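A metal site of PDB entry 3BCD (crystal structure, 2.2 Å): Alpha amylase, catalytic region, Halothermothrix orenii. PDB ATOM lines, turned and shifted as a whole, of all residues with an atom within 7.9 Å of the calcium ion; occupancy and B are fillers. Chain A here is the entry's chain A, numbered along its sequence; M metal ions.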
ATOM      1  N   PRO A 114      31.647   8.937   2.374  1.00  0.00           N
ATOM      2  CA  PRO A 114      30.256   8.761   2.789  1.00  0.00           C
ATOM      3  C   PRO A 114      30.004   7.439   3.486  1.00  0.00           C
ATOM      4  O   PRO A 114      30.654   6.452   3.201  1.00  0.00           O
ATOM      5  CB  PRO A 114      29.484   8.868   1.490  1.00  0.00           C
ATOM      6  CG  PRO A 114      30.392   9.581   0.559  1.00  0.00           C
ATOM      7  CD  PRO A 114      31.777   9.251   0.946  1.00  0.00           C
ATOM      8  N   ILE A 116      27.744   4.644   3.964  1.00  0.00           N
ATOM      9  CA  ILE A 116      26.663   3.929   3.302  1.00  0.00           C
ATOM     10  C   ILE A 116      26.316   2.760   4.200  1.00  0.00           C
ATOM     11  O   ILE A 116      27.213   2.004   4.563  1.00  0.00           O
ATOM     12  CB  ILE A 116      27.093   3.341   1.945  1.00  0.00           C
ATOM     13  CG1 ILE A 116      27.742   4.406   1.039  1.00  0.00           C
ATOM     14  CG2 ILE A 116      25.925   2.622   1.285  1.00  0.00           C
ATOM     15  CD1 ILE A 116      26.929   5.621   0.861  1.00  0.00           C
ATOM     16  N   TYR A 504      30.235   6.365  -3.693  1.00  0.00           N
ATOM     17  CA  TYR A 504      29.529   7.508  -4.313  1.00  0.00           C
ATOM     18  C   TYR A 504      28.347   7.200  -5.256  1.00  0.00           C
ATOM     19  O   TYR A 504      27.418   8.030  -5.379  1.00  0.00           O
ATOM     20  CB  TYR A 504      30.553   8.400  -5.035  1.00  0.00           C
ATOM     21  CG  TYR A 504      31.632   9.022  -4.148  1.00  0.00           C
ATOM     22  CD1 TYR A 504      32.870   8.430  -4.028  1.00  0.00           C
ATOM     23  CD2 TYR A 504      31.414  10.192  -3.450  1.00  0.00           C
ATOM     24  CE1 TYR A 504      33.869   9.000  -3.208  1.00  0.00           C
ATOM     25  CE2 TYR A 504      32.403  10.782  -2.660  1.00  0.00           C
ATOM     26  CZ  TYR A 504      33.633  10.168  -2.545  1.00  0.00           C
ATOM     27  OH  TYR A 504      34.641  10.703  -1.762  1.00  0.00           O
ATOM     28  N   TYR A 506      25.330   6.083  -5.750  1.00  0.00           N
ATOM     29  CA  TYR A 506      24.130   5.732  -4.970  1.00  0.00           C
ATOM     30  C   TYR A 506      22.976   6.669  -5.286  1.00  0.00           C
ATOM     31  O   TYR A 506      23.159   7.711  -5.937  1.00  0.00           O
ATOM     32  CB  TYR A 506      24.451   5.689  -3.488  1.00  0.00           C
ATOM     33  CG  TYR A 506      25.426   4.551  -3.117  1.00  0.00           C
ATOM     34  CD1 TYR A 506      26.783   4.787  -3.005  1.00  0.00           C
ATOM     35  CD2 TYR A 506      24.982   3.269  -2.889  1.00  0.00           C
ATOM     36  CE1 TYR A 506      27.658   3.786  -2.681  1.00  0.00           C
ATOM     37  CE2 TYR A 506      25.864   2.248  -2.602  1.00  0.00           C
ATOM     38  CZ  TYR A 506      27.208   2.511  -2.507  1.00  0.00           C
ATOM     39  OH  TYR A 506      28.090   1.525  -2.165  1.00  0.00           O
ATOM     40  N   GLY A 507      21.759   6.251  -4.891  1.00  0.00           N
ATOM     41  CA  GLY A 507      20.515   6.877  -5.352  1.00  0.00           C
ATOM     42  C   GLY A 507      20.110   6.689  -6.819  1.00  0.00           C
ATOM     43  O   GLY A 507      20.730   5.912  -7.581  1.00  0.00           O
ATOM     44  N   SER A 525      22.446  10.883  -8.120  1.00  0.00           N
ATOM     45  CA  SER A 525      22.095  11.994  -7.265  1.00  0.00           C
ATOM     46  C   SER A 525      22.608  11.832  -5.845  1.00  0.00           C
ATOM     47  O   SER A 525      22.767  12.844  -5.135  1.00  0.00           O
ATOM     48  CB  SER A 525      20.572  12.164  -7.202  1.00  0.00           C
ATOM     49  OG  SER A 525      19.959  11.125  -6.476  1.00  0.00           O
ATOM     50  N   GLY A 526      22.877  10.584  -5.437  1.00  0.00           N
ATOM     51  CA  GLY A 526      23.157  10.257  -4.049  1.00  0.00           C
ATOM     52  C   GLY A 526      21.861   9.943  -3.334  1.00  0.00           C
ATOM     53  O   GLY A 526      20.801  10.293  -3.819  1.00  0.00           O
ATOM     54  N   PHE A 527      21.944   9.271  -2.191  1.00  0.00           N
ATOM     55  CA  PHE A 527      20.795   9.047  -1.277  1.00  0.00           C
ATOM     56  C   PHE A 527      20.482  10.327  -0.535  1.00  0.00           C
ATOM     57  O   PHE A 527      21.401  11.028  -0.125  1.00  0.00           O
ATOM     58  CB  PHE A 527      21.134   8.086  -0.162  1.00  0.00           C
ATOM     59  CG  PHE A 527      21.153   6.613  -0.538  1.00  0.00           C
ATOM     60  CD1 PHE A 527      22.264   5.835  -0.221  1.00  0.00           C
ATOM     61  CD2 PHE A 527      20.053   6.024  -1.118  1.00  0.00           C
ATOM     62  CE1 PHE A 527      22.287   4.476  -0.504  1.00  0.00           C
ATOM     63  CE2 PHE A 527      20.080   4.694  -1.417  1.00  0.00           C
ATOM     64  CZ  PHE A 527      21.203   3.917  -1.107  1.00  0.00           C
ATOM     65  N   PRO A 528      19.205  10.557  -0.221  1.00  0.00           N
ATOM     66  CA  PRO A 528      18.925  11.898   0.271  1.00  0.00           C
ATOM     67  C   PRO A 528      19.261  12.020   1.745  1.00  0.00           C
ATOM     68  O   PRO A 528      19.342  13.128   2.262  1.00  0.00           O
ATOM     69  CB  PRO A 528      17.441  12.066   0.006  1.00  0.00           C
ATOM     70  CG  PRO A 528      16.875  10.640   0.128  1.00  0.00           C
ATOM     71  CD  PRO A 528      18.030   9.681  -0.193  1.00  0.00           C
ATOM     72  N   ASP A 529      19.491  10.867   2.397  1.00  0.00           N
ATOM     73  CA  ASP A 529      19.814  10.802   3.834  1.00  0.00           C
ATOM     74  C   ASP A 529      21.226  10.297   4.127  1.00  0.00           C
ATOM     75  O   ASP A 529      21.491   9.718   5.209  1.00  0.00           O
ATOM     76  CB  ASP A 529      18.784   9.981   4.622  1.00  0.00           C
ATOM     77  CG  ASP A 529      18.108   8.889   3.811  1.00  0.00           C
ATOM     78  OD1 ASP A 529      18.634   8.420   2.759  1.00  0.00           O
ATOM     79  OD2 ASP A 529      16.993   8.485   4.275  1.00  0.00           O
ATOM     80  N   VAL A 530      22.128  10.517   3.176  1.00  0.00           N
ATOM     81  CA  VAL A 530      23.534  10.211   3.356  1.00  0.00           C
ATOM     82  C   VAL A 530      24.265  11.422   2.851  1.00  0.00           C
ATOM     83  O   VAL A 530      23.902  11.953   1.803  1.00  0.00           O
ATOM     84  CB  VAL A 530      24.003   8.909   2.599  1.00  0.00           C
ATOM     85  CG1 VAL A 530      25.489   8.698   2.797  1.00  0.00           C
ATOM     86  CG2 VAL A 530      23.194   7.709   3.066  1.00  0.00           C
ATOM     87  N   ALA A 531      25.257  11.884   3.591  1.00  0.00           N
ATOM     88  CA  ALA A 531      25.920  13.094   3.271  1.00  0.00           C
ATOM     89  C   ALA A 531      27.117  12.753   2.404  1.00  0.00           C
ATOM     90  O   ALA A 531      27.846  11.776   2.646  1.00  0.00           O
ATOM     91  CB  ALA A 531      26.330  13.824   4.548  1.00  0.00           C
ATOM     92  N   GLY A 532      27.297  13.509   1.330  1.00  0.00           N
ATOM     93  CA  GLY A 532      28.543  13.460   0.587  1.00  0.00           C
ATOM     94  C   GLY A 532      28.678  12.478  -0.570  1.00  0.00           C
ATOM     95  O   GLY A 532      29.792  12.312  -1.107  1.00  0.00           O
ATOM     96  N   ASP A 533      27.561  11.837  -0.944  1.00  0.00           N
ATOM     97  CA  ASP A 533      27.509  10.796  -1.995  1.00  0.00           C
ATOM     98  C   ASP A 533      26.962  11.338  -3.332  1.00  0.00           C
ATOM     99  O   ASP A 533      26.641  12.552  -3.459  1.00  0.00           O
ATOM    100  CB  ASP A 533      26.733   9.529  -1.541  1.00  0.00           C
ATOM    101  CG  ASP A 533      25.280   9.794  -1.271  1.00  0.00           C
ATOM    102  OD1 ASP A 533      24.935  10.984  -1.109  1.00  0.00           O
ATOM    103  OD2 ASP A 533      24.472   8.829  -1.232  1.00  0.00           O
ATOM    104  N   GLY A 534      26.925  10.471  -4.346  1.00  0.00           N
ATOM    105  CA  GLY A 534      26.493  10.899  -5.647  1.00  0.00           C
ATOM    106  C   GLY A 534      27.653  11.252  -6.542  1.00  0.00           C
ATOM    107  O   GLY A 534      28.748  11.434  -6.078  1.00  0.00           O
ATOM    108  N   ARG A 555      21.765  17.603  -9.359  1.00  0.00           N
ATOM    109  CA  ARG A 555      20.764  17.306  -8.326  1.00  0.00           C
ATOM    110  C   ARG A 555      21.240  17.609  -6.896  1.00  0.00           C
ATOM    111  O   ARG A 555      20.611  17.203  -5.921  1.00  0.00           O
ATOM    112  CB  ARG A 555      20.275  15.846  -8.426  1.00  0.00           C
ATOM    113  CG  ARG A 555      19.075  15.658  -9.391  1.00  0.00           C
ATOM    114  CD  ARG A 555      19.431  15.901 -10.868  1.00  0.00           C
ATOM    115  NE  ARG A 555      18.269  15.596 -11.686  1.00  0.00           N
ATOM    116  CZ  ARG A 555      18.295  15.349 -13.005  1.00  0.00           C
ATOM    117  NH1 ARG A 555      19.425  15.385 -13.702  1.00  0.00           N
ATOM    118  NH2 ARG A 555      17.153  15.047 -13.640  1.00  0.00           N
ATOM    119  N   GLN A 556      22.367  18.330  -6.795  1.00  0.00           N
ATOM    120  CA  GLN A 556      22.918  18.786  -5.518  1.00  0.00           C
ATOM    121  C   GLN A 556      23.262  20.255  -5.649  1.00  0.00           C
ATOM    122  O   GLN A 556      24.348  20.613  -6.116  1.00  0.00           O
ATOM    123  CB  GLN A 556      24.172  18.011  -5.177  1.00  0.00           C
ATOM    124  CG  GLN A 556      23.951  16.522  -5.021  1.00  0.00           C
ATOM    125  CD  GLN A 556      25.097  15.841  -4.308  1.00  0.00           C
ATOM    126  OE1 GLN A 556      25.313  16.062  -3.118  1.00  0.00           O
ATOM    127  NE2 GLN A 556      25.838  15.008  -5.041  1.00  0.00           N
ATOM    128  N   PRO A 597      31.399  14.922  -4.662  1.00  0.00           N
ATOM    129  CA  PRO A 597      31.505  16.013  -3.677  1.00  0.00           C
ATOM    130  C   PRO A 597      32.824  16.009  -2.821  1.00  0.00           C
ATOM    131  O   PRO A 597      33.399  14.928  -2.499  1.00  0.00           O
ATOM    132  CB  PRO A 597      30.246  15.818  -2.808  1.00  0.00           C
ATOM    133  CG  PRO A 597      29.356  14.921  -3.505  1.00  0.00           C
ATOM    134  CD  PRO A 597      30.284  14.018  -4.311  1.00  0.00           C
HETATM  135 CA    CA M   1      23.231  12.429  -0.523  1.00  0.00          CA
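O of Asp 533 lies within hydrogen-bond range of NE2 of Gln 556, 3.0 Å away.
The backbone carbonyl oxygen of Tyr 506 is in hydrogen-bond range of the backbone NH of Gly 526, 2.9 Å away.
Gly 526 touches the calcium ion.
Within 4 Å of the calcium ion: Gly 526, Phe 527, Val 530 and Asp 533.
The nearest printed residue that does not touch the calcium ion is Pro 528 (4.4 Å).
The calcium ion is bound by OD1 of Asp 533, 2.3 Å away.
O of Phe 527 is bound to the calcium ion (2.3 Å).
The calcium ion is bound by the backbone carbonyl oxygen (O) of Val 530 (2.5 Å).
The calcium ion has three donor atoms within binding distance.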
